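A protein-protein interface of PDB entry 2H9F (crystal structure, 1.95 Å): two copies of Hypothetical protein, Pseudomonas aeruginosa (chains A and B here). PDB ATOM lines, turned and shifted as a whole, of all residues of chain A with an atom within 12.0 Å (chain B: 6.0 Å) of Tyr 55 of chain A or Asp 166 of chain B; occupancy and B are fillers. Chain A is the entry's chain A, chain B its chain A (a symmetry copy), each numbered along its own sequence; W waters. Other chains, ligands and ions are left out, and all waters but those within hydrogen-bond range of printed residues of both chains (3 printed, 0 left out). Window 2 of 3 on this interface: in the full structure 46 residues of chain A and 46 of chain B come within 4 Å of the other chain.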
ATOM      1  N   ARG A  47     -10.901   0.610 -16.762  1.00  0.00           N
ATOM      2  CA  ARG A  47     -10.501   1.644 -15.805  1.00  0.00           C
ATOM      3  C   ARG A  47      -8.974   1.670 -15.623  1.00  0.00           C
ATOM      4  O   ARG A  47      -8.353   2.757 -15.508  1.00  0.00           O
ATOM      5  CB  ARG A  47     -11.293   1.464 -14.492  1.00  0.00           C
ATOM      6  CG  ARG A  47     -11.263   2.675 -13.545  1.00  0.00           C
ATOM      7  CD  ARG A  47     -12.153   3.885 -13.959  1.00  0.00           C
ATOM      8  NE  ARG A  47     -11.387   5.044 -13.531  1.00  0.00           N
ATOM      9  CZ  ARG A  47     -11.710   5.965 -12.624  1.00  0.00           C
ATOM     10  NH1 ARG A  47     -12.906   6.058 -12.025  1.00  0.00           N
ATOM     11  NH2 ARG A  47     -10.777   6.877 -12.367  1.00  0.00           N
ATOM     12  N   ILE A  49      -6.770   0.949 -17.864  1.00  0.00           N
ATOM     13  CA  ILE A  49      -6.316   1.590 -19.098  1.00  0.00           C
ATOM     14  C   ILE A  49      -6.617   3.083 -19.223  1.00  0.00           C
ATOM     15  O   ILE A  49      -5.758   3.858 -19.718  1.00  0.00           O
ATOM     16  CB  ILE A  49      -6.804   0.839 -20.349  1.00  0.00           C
ATOM     17  CG1 ILE A  49      -6.038  -0.495 -20.462  1.00  0.00           C
ATOM     18  CG2 ILE A  49      -6.598   1.663 -21.621  1.00  0.00           C
ATOM     19  CD1 ILE A  49      -4.503  -0.359 -20.475  1.00  0.00           C
ATOM     20  N   GLY A  50      -7.745   3.484 -18.664  1.00  0.00           N
ATOM     21  CA  GLY A  50      -8.166   4.884 -18.642  1.00  0.00           C
ATOM     22  C   GLY A  50      -9.258   5.180 -19.660  1.00  0.00           C
ATOM     23  O   GLY A  50      -9.392   6.331 -20.106  1.00  0.00           O
ATOM     24  N   SER A  51     -10.006   4.138 -20.008  1.00  0.00           N
ATOM     25  CA  SER A  51     -11.082   4.197 -20.987  1.00  0.00           C
ATOM     26  C   SER A  51     -12.419   4.035 -20.289  1.00  0.00           C
ATOM     27  O   SER A  51     -12.491   3.560 -19.156  1.00  0.00           O
ATOM     28  CB  SER A  51     -10.930   3.051 -22.015  1.00  0.00           C
ATOM     29  OG  SER A  51      -9.783   3.213 -22.821  1.00  0.00           O
ATOM     30  N   PRO A  52     -13.493   4.453 -20.951  1.00  0.00           N
ATOM     31  CA  PRO A  52     -13.546   5.178 -22.238  1.00  0.00           C
ATOM     32  C   PRO A  52     -13.148   6.642 -22.034  1.00  0.00           C
ATOM     33  O   PRO A  52     -13.599   7.247 -21.087  1.00  0.00           O
ATOM     34  CB  PRO A  52     -15.011   5.089 -22.645  1.00  0.00           C
ATOM     35  CG  PRO A  52     -15.738   4.960 -21.387  1.00  0.00           C
ATOM     36  CD  PRO A  52     -14.834   4.212 -20.406  1.00  0.00           C
ATOM     37  N   ASP A  53     -12.279   7.154 -22.898  1.00  0.00           N
ATOM     38  CA  ASP A  53     -11.771   8.492 -22.790  1.00  0.00           C
ATOM     39  C   ASP A  53     -12.191   9.374 -23.987  1.00  0.00           C
ATOM     40  O   ASP A  53     -11.714   9.185 -25.100  1.00  0.00           O
ATOM     41  CB  ASP A  53     -10.259   8.456 -22.728  1.00  0.00           C
ATOM     42  CG  ASP A  53      -9.663   9.822 -22.533  1.00  0.00           C
ATOM     43  OD1 ASP A  53     -10.406  10.727 -22.080  1.00  0.00           O
ATOM     44  OD2 ASP A  53      -8.469   9.991 -22.784  1.00  0.00           O
ATOM     45  N   PRO A  54     -13.039  10.375 -23.739  1.00  0.00           N
ATOM     46  CA  PRO A  54     -13.464  11.349 -24.741  1.00  0.00           C
ATOM     47  C   PRO A  54     -12.320  12.217 -25.256  1.00  0.00           C
ATOM     48  O   PRO A  54     -12.371  12.724 -26.360  1.00  0.00           O
ATOM     49  CB  PRO A  54     -14.411  12.241 -23.954  1.00  0.00           C
ATOM     50  CG  PRO A  54     -14.777  11.487 -22.784  1.00  0.00           C
ATOM     51  CD  PRO A  54     -13.623  10.678 -22.434  1.00  0.00           C
ATOM     52  N   TYR A  55     -11.300  12.390 -24.445  1.00  0.00           N
ATOM     53  CA  TYR A  55     -10.116  13.129 -24.872  1.00  0.00           C
ATOM     54  C   TYR A  55      -9.149  12.302 -25.728  1.00  0.00           C
ATOM     55  O   TYR A  55      -8.180  12.822 -26.269  1.00  0.00           O
ATOM     56  CB  TYR A  55      -9.410  13.620 -23.639  1.00  0.00           C
ATOM     57  CG  TYR A  55     -10.293  14.437 -22.698  1.00  0.00           C
ATOM     58  CD1 TYR A  55     -10.684  15.724 -23.031  1.00  0.00           C
ATOM     59  CD2 TYR A  55     -10.740  13.912 -21.487  1.00  0.00           C
ATOM     60  CE1 TYR A  55     -11.484  16.474 -22.199  1.00  0.00           C
ATOM     61  CE2 TYR A  55     -11.547  14.652 -20.643  1.00  0.00           C
ATOM     62  CZ  TYR A  55     -11.918  15.941 -21.003  1.00  0.00           C
ATOM     63  OH  TYR A  55     -12.683  16.732 -20.149  1.00  0.00           O
ATOM     64  N   ALA A  56      -9.368  10.994 -25.805  1.00  0.00           N
ATOM     65  CA  ALA A  56      -8.519  10.158 -26.613  1.00  0.00           C
ATOM     66  C   ALA A  56      -7.040  10.315 -26.271  1.00  0.00           C
ATOM     67  O   ALA A  56      -6.228  10.294 -27.181  1.00  0.00           O
ATOM     68  CB  ALA A  56      -8.773  10.467 -28.143  1.00  0.00           C
ATOM     69  N   ALA A  57      -6.684  10.422 -24.982  1.00  0.00           N
ATOM     70  CA  ALA A  57      -5.302  10.698 -24.564  1.00  0.00           C
ATOM     71  C   ALA A  57      -4.804   9.778 -23.437  1.00  0.00           C
ATOM     72  O   ALA A  57      -3.602   9.675 -23.207  1.00  0.00           O
ATOM     73  CB  ALA A  57      -5.209  12.164 -24.130  1.00  0.00           C
ATOM     74  N   HIS A  58      -5.725   9.089 -22.762  1.00  0.00           N
ATOM     75  CA  HIS A  58      -5.385   8.169 -21.662  1.00  0.00           C
ATOM     76  C   HIS A  58      -4.467   8.827 -20.603  1.00  0.00           C
ATOM     77  O   HIS A  58      -3.503   8.224 -20.098  1.00  0.00           O
ATOM     78  CB  HIS A  58      -4.765   6.894 -22.209  1.00  0.00           C
ATOM     79  CG  HIS A  58      -5.767   5.931 -22.753  1.00  0.00           C
ATOM     80  ND1 HIS A  58      -5.423   4.912 -23.606  1.00  0.00           N
ATOM     81  CD2 HIS A  58      -7.088   5.802 -22.514  1.00  0.00           C
ATOM     82  CE1 HIS A  58      -6.498   4.189 -23.869  1.00  0.00           C
ATOM     83  NE2 HIS A  58      -7.525   4.722 -23.232  1.00  0.00           N
ATOM     84  N   ILE A  59      -4.777  10.072 -20.276  1.00  0.00           N
ATOM     85  CA  ILE A  59      -4.061  10.773 -19.236  1.00  0.00           C
ATOM     86  C   ILE A  59      -4.454  10.237 -17.871  1.00  0.00           C
ATOM     87  O   ILE A  59      -3.711  10.374 -16.945  1.00  0.00           O
ATOM     88  CB  ILE A  59      -4.235  12.299 -19.355  1.00  0.00           C
ATOM     89  CG1 ILE A  59      -3.390  12.838 -20.531  1.00  0.00           C
ATOM     90  CG2 ILE A  59      -3.777  12.997 -18.131  1.00  0.00           C
ATOM     91  CD1 ILE A  59      -1.873  12.753 -20.351  1.00  0.00           C
ATOM     92  N   ASP A  60      -5.582   9.554 -17.770  1.00  0.00           N
ATOM     93  CA  ASP A  60      -6.018   9.054 -16.482  1.00  0.00           C
ATOM     94  C   ASP A  60      -6.023   7.526 -16.429  1.00  0.00           C
ATOM     95  O   ASP A  60      -6.921   6.924 -15.887  1.00  0.00           O
ATOM     96  CB  ASP A  60      -7.398   9.597 -16.184  1.00  0.00           C
ATOM     97  CG  ASP A  60      -7.722   9.631 -14.696  1.00  0.00           C
ATOM     98  OD1 ASP A  60      -6.838   9.529 -13.829  1.00  0.00           O
ATOM     99  OD2 ASP A  60      -8.887   9.772 -14.370  1.00  0.00           O
ATOM    100  N   GLY A  61      -4.988   6.927 -17.002  1.00  0.00           N
ATOM    101  CA  GLY A  61      -4.807   5.506 -16.906  1.00  0.00           C
ATOM    102  C   GLY A  61      -3.524   5.024 -17.490  1.00  0.00           C
ATOM    103  O   GLY A  61      -2.575   5.816 -17.775  1.00  0.00           O
ATOM    104  N   GLY A  63      -3.068   3.285 -20.187  1.00  0.00           N
ATOM    105  CA  GLY A  63      -3.049   3.316 -21.641  1.00  0.00           C
ATOM    106  C   GLY A  63      -2.145   4.407 -22.196  1.00  0.00           C
ATOM    107  O   GLY A  63      -1.720   5.347 -21.497  1.00  0.00           O
ATOM    108  N   GLY A  64      -1.810   4.264 -23.473  1.00  0.00           N
ATOM    109  CA  GLY A  64      -1.051   5.298 -24.183  1.00  0.00           C
ATOM    110  C   GLY A  64      -1.831   5.850 -25.372  1.00  0.00           C
ATOM    111  O   GLY A  64      -1.258   6.460 -26.245  1.00  0.00           O
ATOM    112  N   ALA A  65      -3.143   5.641 -25.377  1.00  0.00           N
ATOM    113  CA  ALA A  65      -4.047   6.160 -26.405  1.00  0.00           C
ATOM    114  C   ALA A  65      -3.720   5.716 -27.849  1.00  0.00           C
ATOM    115  O   ALA A  65      -4.088   6.400 -28.806  1.00  0.00           O
ATOM    116  CB  ALA A  65      -4.200   7.707 -26.296  1.00  0.00           C
ATOM    117  N   THR A  66      -3.058   4.569 -27.994  1.00  0.00           N
ATOM    118  CA  THR A  66      -2.905   3.894 -29.284  1.00  0.00           C
ATOM    119  C   THR A  66      -3.313   2.434 -29.177  1.00  0.00           C
ATOM    120  O   THR A  66      -3.408   1.875 -28.082  1.00  0.00           O
ATOM    121  CB  THR A  66      -1.487   3.961 -29.798  1.00  0.00           C
ATOM    122  OG1 THR A  66      -0.659   3.105 -29.011  1.00  0.00           O
ATOM    123  CG2 THR A  66      -0.994   5.400 -29.777  1.00  0.00           C
ATOM    124  N   SER A  70      -3.070  -0.151 -25.540  1.00  0.00           N
ATOM    125  CA  SER A  70      -4.354  -0.168 -24.893  1.00  0.00           C
ATOM    126  C   SER A  70      -4.793  -1.617 -24.687  1.00  0.00           C
ATOM    127  O   SER A  70      -5.810  -2.074 -25.180  1.00  0.00           O
ATOM    128  CB  SER A  70      -5.353   0.680 -25.669  1.00  0.00           C
ATOM    129  OG  SER A  70      -6.626   0.639 -25.037  1.00  0.00           O
ATOM    130  N   SER A  93     -10.893  -0.624 -26.005  1.00  0.00           N
ATOM    131  CA  SER A  93     -11.201   0.500 -26.888  1.00  0.00           C
ATOM    132  C   SER A  93     -10.856   1.828 -26.214  1.00  0.00           C
ATOM    133  O   SER A  93     -10.975   1.966 -25.001  1.00  0.00           O
ATOM    134  CB  SER A  93     -12.673   0.469 -27.267  1.00  0.00           C
ATOM    135  OG  SER A  93     -13.049   1.688 -27.861  1.00  0.00           O
ATOM    136  N   ILE A  94     -10.420   2.807 -26.988  1.00  0.00           N
ATOM    137  CA  ILE A  94      -9.933   4.069 -26.397  1.00  0.00           C
ATOM    138  C   ILE A  94     -11.130   4.927 -26.028  1.00  0.00           C
ATOM    139  O   ILE A  94     -11.208   5.465 -24.933  1.00  0.00           O
ATOM    140  CB  ILE A  94      -8.978   4.822 -27.329  1.00  0.00           C
ATOM    141  CG1 ILE A  94      -7.717   3.969 -27.541  1.00  0.00           C
ATOM    142  CG2 ILE A  94      -8.632   6.266 -26.748  1.00  0.00           C
ATOM    143  CD1 ILE A  94      -6.747   4.477 -28.610  1.00  0.00           C
ATOM    144  N   ASP A  95     -12.085   4.977 -26.937  1.00  0.00           N
ATOM    145  CA  ASP A  95     -13.151   5.941 -26.872  1.00  0.00           C
ATOM    146  C   ASP A  95     -14.524   5.333 -26.572  1.00  0.00           C
ATOM    147  O   ASP A  95     -15.440   6.067 -26.217  1.00  0.00           O
ATOM    148  CB  ASP A  95     -13.201   6.675 -28.212  1.00  0.00           C
ATOM    149  CG  ASP A  95     -13.704   5.796 -29.342  1.00  0.00           C
ATOM    150  OD1 ASP A  95     -13.231   4.642 -29.521  1.00  0.00           O
ATOM    151  OD2 ASP A  95     -14.581   6.277 -30.076  1.00  0.00           O
ATOM    152  N   LYS A  96     -14.662   4.020 -26.707  1.00  0.00           N
ATOM    153  CA  LYS A  96     -15.894   3.331 -26.351  1.00  0.00           C
ATOM    154  C   LYS A  96     -15.622   2.418 -25.142  1.00  0.00           C
ATOM    155  O   LYS A  96     -14.462   2.028 -24.864  1.00  0.00           O
ATOM    156  CB  LYS A  96     -16.469   2.558 -27.562  1.00  0.00           C
ATOM    157  CG  LYS A  96     -16.886   3.521 -28.719  1.00  0.00           C
ATOM    158  CD  LYS A  96     -17.487   2.828 -29.983  1.00  0.00           C
ATOM    159  N   PRO A  97     -16.686   2.128 -24.364  1.00  0.00           N
ATOM    160  CA  PRO A  97     -16.528   1.180 -23.258  1.00  0.00           C
ATOM    161  C   PRO A  97     -16.661  -0.231 -23.795  1.00  0.00           C
ATOM    162  O   PRO A  97     -17.768  -0.757 -23.897  1.00  0.00           O
ATOM    163  CB  PRO A  97     -17.674   1.554 -22.323  1.00  0.00           C
ATOM    164  CG  PRO A  97     -18.760   2.023 -23.261  1.00  0.00           C
ATOM    165  CD  PRO A  97     -18.073   2.639 -24.456  1.00  0.00           C
ATOM    166  N   THR B  19      -3.385  17.354 -15.748  1.00  0.00           N
ATOM    167  CA  THR B  19      -3.631  16.803 -17.092  1.00  0.00           C
ATOM    168  C   THR B  19      -2.333  16.234 -17.715  1.00  0.00           C
ATOM    169  O   THR B  19      -2.246  16.111 -18.942  1.00  0.00           O
ATOM    170  CB  THR B  19      -4.247  17.874 -18.031  1.00  0.00           C
ATOM    171  OG1 THR B  19      -3.382  19.012 -18.031  1.00  0.00           O
ATOM    172  CG2 THR B  19      -5.626  18.300 -17.576  1.00  0.00           C
ATOM    173  N   GLU B 164     -14.274  17.541 -10.938  1.00  0.00           N
ATOM    174  CA  GLU B 164     -13.960  17.401 -12.362  1.00  0.00           C
ATOM    175  C   GLU B 164     -12.946  18.427 -12.800  1.00  0.00           C
ATOM    176  O   GLU B 164     -13.022  19.596 -12.422  1.00  0.00           O
ATOM    177  CB  GLU B 164     -15.187  17.626 -13.234  1.00  0.00           C
ATOM    178  CG  GLU B 164     -16.268  16.548 -13.282  1.00  0.00           C
ATOM    179  CD  GLU B 164     -17.538  17.000 -14.073  1.00  0.00           C
ATOM    180  N   LEU B 165     -12.005  17.997 -13.637  1.00  0.00           N
ATOM    181  CA  LEU B 165     -11.031  18.880 -14.224  1.00  0.00           C
ATOM    182  C   LEU B 165     -11.054  18.620 -15.729  1.00  0.00           C
ATOM    183  O   LEU B 165     -10.960  17.472 -16.154  1.00  0.00           O
ATOM    184  CB  LEU B 165      -9.656  18.585 -13.642  1.00  0.00           C
ATOM    185  CG  LEU B 165      -8.507  19.507 -14.061  1.00  0.00           C
ATOM    186  CD1 LEU B 165      -8.757  20.922 -13.567  1.00  0.00           C
ATOM    187  CD2 LEU B 165      -7.227  18.909 -13.521  1.00  0.00           C
ATOM    188  N   ASP B 166     -11.195  19.678 -16.526  1.00  0.00           N
ATOM    189  CA  ASP B 166     -11.116  19.568 -17.970  1.00  0.00           C
ATOM    190  C   ASP B 166      -9.835  18.841 -18.389  1.00  0.00           C
ATOM    191  O   ASP B 166      -8.741  19.135 -17.904  1.00  0.00           O
ATOM    192  CB  ASP B 166     -11.232  20.950 -18.641  1.00  0.00           C
ATOM    193  CG  ASP B 166     -11.289  20.878 -20.197  1.00  0.00           C
ATOM    194  OD1 ASP B 166     -12.239  20.296 -20.758  1.00  0.00           O
ATOM    195  OD2 ASP B 166     -10.386  21.448 -20.853  1.00  0.00           O
ATOM    196  N   GLY B 167      -9.996  17.877 -19.287  1.00  0.00           N
ATOM    197  CA  GLY B 167      -8.871  17.028 -19.739  1.00  0.00           C
ATOM    198  C   GLY B 167      -8.583  15.807 -18.890  1.00  0.00           C
ATOM    199  O   GLY B 167      -7.730  15.002 -19.252  1.00  0.00           O
ATOM    200  N   VAL B 168      -9.267  15.681 -17.748  1.00  0.00           N
ATOM    201  CA  VAL B 168      -9.208  14.471 -16.893  1.00  0.00           C
ATOM    202  C   VAL B 168     -10.499  13.716 -17.006  1.00  0.00           C
ATOM    203  O   VAL B 168     -11.561  14.171 -16.636  1.00  0.00           O
ATOM    204  CB  VAL B 168      -8.953  14.836 -15.436  1.00  0.00           C
ATOM    205  CG1 VAL B 168      -8.923  13.599 -14.524  1.00  0.00           C
ATOM    206  CG2 VAL B 168      -7.639  15.610 -15.352  1.00  0.00           C
ATOM    207  N   THR B 169     -10.368  12.510 -17.511  1.00  0.00           N
ATOM    208  CA  THR B 169     -11.475  11.701 -17.883  1.00  0.00           C
ATOM    209  C   THR B 169     -12.396  11.463 -16.695  1.00  0.00           C
ATOM    210  O   THR B 169     -13.593  11.580 -16.811  1.00  0.00           O
ATOM    211  CB  THR B 169     -10.897  10.339 -18.425  1.00  0.00           C
ATOM    212  OG1 THR B 169      -9.799  10.592 -19.327  1.00  0.00           O
ATOM    213  CG2 THR B 169     -11.985   9.527 -19.069  1.00  0.00           C
ATOM    214  N   HIS B 314     -12.452  29.756 -27.591  1.00  0.00           N
ATOM    215  CA  HIS B 314     -12.002  28.561 -26.868  1.00  0.00           C
ATOM    216  C   HIS B 314     -13.188  27.830 -26.231  1.00  0.00           C
ATOM    217  O   HIS B 314     -14.132  28.465 -25.814  1.00  0.00           O
ATOM    218  CB  HIS B 314     -10.996  28.962 -25.814  1.00  0.00           C
ATOM    219  CG  HIS B 314     -10.194  27.821 -25.274  1.00  0.00           C
ATOM    220  ND1 HIS B 314     -10.673  26.969 -24.304  1.00  0.00           N
ATOM    221  CD2 HIS B 314      -8.932  27.411 -25.550  1.00  0.00           C
ATOM    222  CE1 HIS B 314      -9.749  26.074 -24.014  1.00  0.00           C
ATOM    223  NE2 HIS B 314      -8.678  26.327 -24.748  1.00  0.00           N
ATOM    224  N   HIS B 315     -13.127  26.495 -26.165  1.00  0.00           N
ATOM    225  CA  HIS B 315     -14.237  25.636 -25.685  1.00  0.00           C
ATOM    226  C   HIS B 315     -14.467  25.691 -24.178  1.00  0.00           C
ATOM    227  O   HIS B 315     -15.538  25.288 -23.673  1.00  0.00           O
ATOM    228  CB  HIS B 315     -14.018  24.136 -26.090  1.00  0.00           C
ATOM    229  CG  HIS B 315     -13.039  23.382 -25.218  1.00  0.00           C
ATOM    230  ND1 HIS B 315     -11.665  23.543 -25.309  1.00  0.00           N
ATOM    231  CD2 HIS B 315     -13.242  22.468 -24.236  1.00  0.00           C
ATOM    232  CE1 HIS B 315     -11.071  22.763 -24.416  1.00  0.00           C
ATOM    233  NE2 HIS B 315     -12.006  22.104 -23.749  1.00  0.00           N
ATOM    234  N   ALA B 316     -13.444  26.109 -23.462  1.00  0.00           N
ATOM    235  CA  ALA B 316     -13.491  26.221 -22.028  1.00  0.00           C
ATOM    236  C   ALA B 316     -12.645  27.472 -21.665  1.00  0.00           C
ATOM    237  O   ALA B 316     -13.008  28.590 -22.023  1.00  0.00           O
ATOM    238  CB  ALA B 316     -12.955  24.936 -21.408  1.00  0.00           C
ATOM    239  N   MET B 317     -11.519  27.309 -20.992  1.00  0.00           N
ATOM    240  CA  MET B 317     -10.632  28.453 -20.814  1.00  0.00           C
ATOM    241  C   MET B 317      -9.183  28.003 -20.847  1.00  0.00           C
ATOM    242  O   MET B 317      -8.847  26.961 -20.315  1.00  0.00           O
ATOM    243  CB  MET B 317     -10.980  29.170 -19.494  1.00  0.00           C
ATOM    244  CG  MET B 317     -10.245  30.475 -19.263  1.00  0.00           C
ATOM    245  SD  MET B 317     -10.526  31.808 -20.672  1.00  0.00           S
ATOM    246  CE  MET B 317     -12.488  31.667 -20.671  1.00  0.00           C
ATOM    247  N   SER B 354     -18.183  25.451 -21.720  1.00  0.00           N
ATOM    248  CA  SER B 354     -18.399  24.044 -21.433  1.00  0.00           C
ATOM    249  C   SER B 354     -18.592  23.687 -19.942  1.00  0.00           C
ATOM    250  O   SER B 354     -18.660  22.507 -19.562  1.00  0.00           O
ATOM    251  CB  SER B 354     -17.271  23.217 -22.073  1.00  0.00           C
ATOM    252  OG  SER B 354     -16.032  23.505 -21.516  1.00  0.00           O
HETATM  253  O   HOH W   1      -7.871   8.585 -19.474  1.00  0.00           O
HETATM  254  O   HOH W   2     -13.645  15.685 -17.965  1.00  0.00           O
HETATM  255  O   HOH W   3      -7.105  11.653 -21.155  1.00  0.00           O
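OD1 of Asp 53 of chain A sits at hydrogen-bond distance from OG1 of Thr 169 of chain B (2.8 Å). N of Gly 167 of chain B is in hydrogen-bond range of OH of Tyr 55 of chain A (3.0 Å).
NH2 of Arg 47 of chain A is in salt-bridge range of OD2 of Asp 60 of chain A, at 3.996 Å. The side-chain carboxylate of Asp 53 of chain A is in hydrogen-bond range of the backbone NH of Ala 57 of chain A (2.9 Å). NE2 of His 315 of chain B sits at hydrogen-bond distance from OD2 of Asp 166 of chain B, 3.4 Å away. The side-chain carboxylate of Asp 53 of chain A lies within hydrogen-bond range of the backbone NH of Ala 56 of chain A. OD2 of Asp 53 of chain A is in hydrogen-bond range of N of His 58 of chain A, 2.9 Å away. The side-chain carboxylate (OD1) of Asp 53 of chain A sits at hydrogen-bond distance from the backbone NH (N) of Tyr 55 of chain A (3.0 Å).
Among the printed residues, merely in contact across the chains: Pro 52 of chain A with Thr 169 of chain B (3.4 Å), Pro 54 of chain A with Thr 169 of chain B (3.9 Å), Tyr 55 of chain A with Asp 166 of chain B (3.6 Å), Tyr 55 of chain A with Val 168 of chain B (3.8 Å), Tyr 55 of chain A with Thr 169 of chain B (3.97 Å), Ile 59 of chain A with Thr 19 of chain B (3.6 Å) and Asp 60 of chain A with Val 168 of chain B (3.8 Å).
Printed residues of chain B within 4 Å of Pro 52 of chain A: Thr 169 (3.4 Å). Of the printed residues of chain B, Asp 53 of chain A touches Thr 169 (2.8 Å). Printed residues of chain B within 4 Å of Pro 54 of chain A: Thr 169. Tyr 55 of chain A touches just these residues of chain B: Asp 166, Gly 167, Val 168 and Thr 169. Of the printed residues of chain B, Ile 59 of chain A touches Thr 19 (3.6 Å). Of the printed residues of chain B, Asp 60 of chain A touches Val 168. Ser 93 of chain A touches none of the printed residues of chain B. Thr 19 of chain B touches just one residue of chain A: Ile 59 (3.6 Å). No residue of chain A comes within 4 Å of Glu 164 of chain B. No residue of chain A comes within 4 Å of Leu 165 of chain B. Of chain A, only Tyr 55 comes within 4 Å of Asp 166 of chain B. Gly 167 of chain B touches just one residue of chain A: Tyr 55. Of chain A, only Tyr 55 (3.8 Å) and Asp 60 (3.8 Å) come within 4 Å of Val 168 of chain B. Thr 169 of chain B touches just these residues of chain A: Pro 52 (3.4 Å), Asp 53 (2.8 Å), Pro 54 (3.9 Å) and Tyr 55 (3.97 Å). No residue of chain A comes within 4 Å of Ala 316 of chain B. The nearest residue of chain A that does not touch Asp 166 of chain B is Ile 59 of chain A (7.9 Å). The nearest printed residue of chain B that does not touch Asp 53 of chain A is Gly 167 of chain B (5.8 Å).
Of the 12 printed residues of chain B, 5 touch a printed residue of chain A. Printed residues of chain B that touch a printed residue of chain A: Thr 19, Asp 166, Gly 167, Val 168 and Thr 169. Of the 24 printed residues of chain A, 6 touch a printed residue of chain B. Hydrophobic or aromatic side chains of chain A that line the printed part of chain B: Pro 54, Tyr 55 and Ile 59. Among the printed residues, no Asp or Glu carboxylate lies within 4 Å of a Lys or Arg side-chain nitrogen of the other chain.
No position is printed for both chains. Of the 9 pairs that touch across the chains among the printed residues, none has its exchanged pair printed and touching as well.
Water W2 lies within hydrogen-bond range of OH of Tyr 55 of chain A (2.6 Å) and O of Val 168 of chain B (2.9 Å). Water W3 lies within hydrogen-bond range of OD2 of Asp 53 of chain A (2.7 Å), N of Ile 59 of chain A (2.9 Å), N of His 58 of chain A (3.3 Å) and OG1 of Thr 169 of chain B (3.4 Å). Water W1 lies within hydrogen-bond range of the side-chain hydroxyl (OG1) of Thr 169 of chain B (2.8 Å), the backbone carbonyl oxygen (O) of Gly 50 of chain A (2.8 Å) and the backbone NH (N) of Asp 60 of chain A (3.0 Å).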
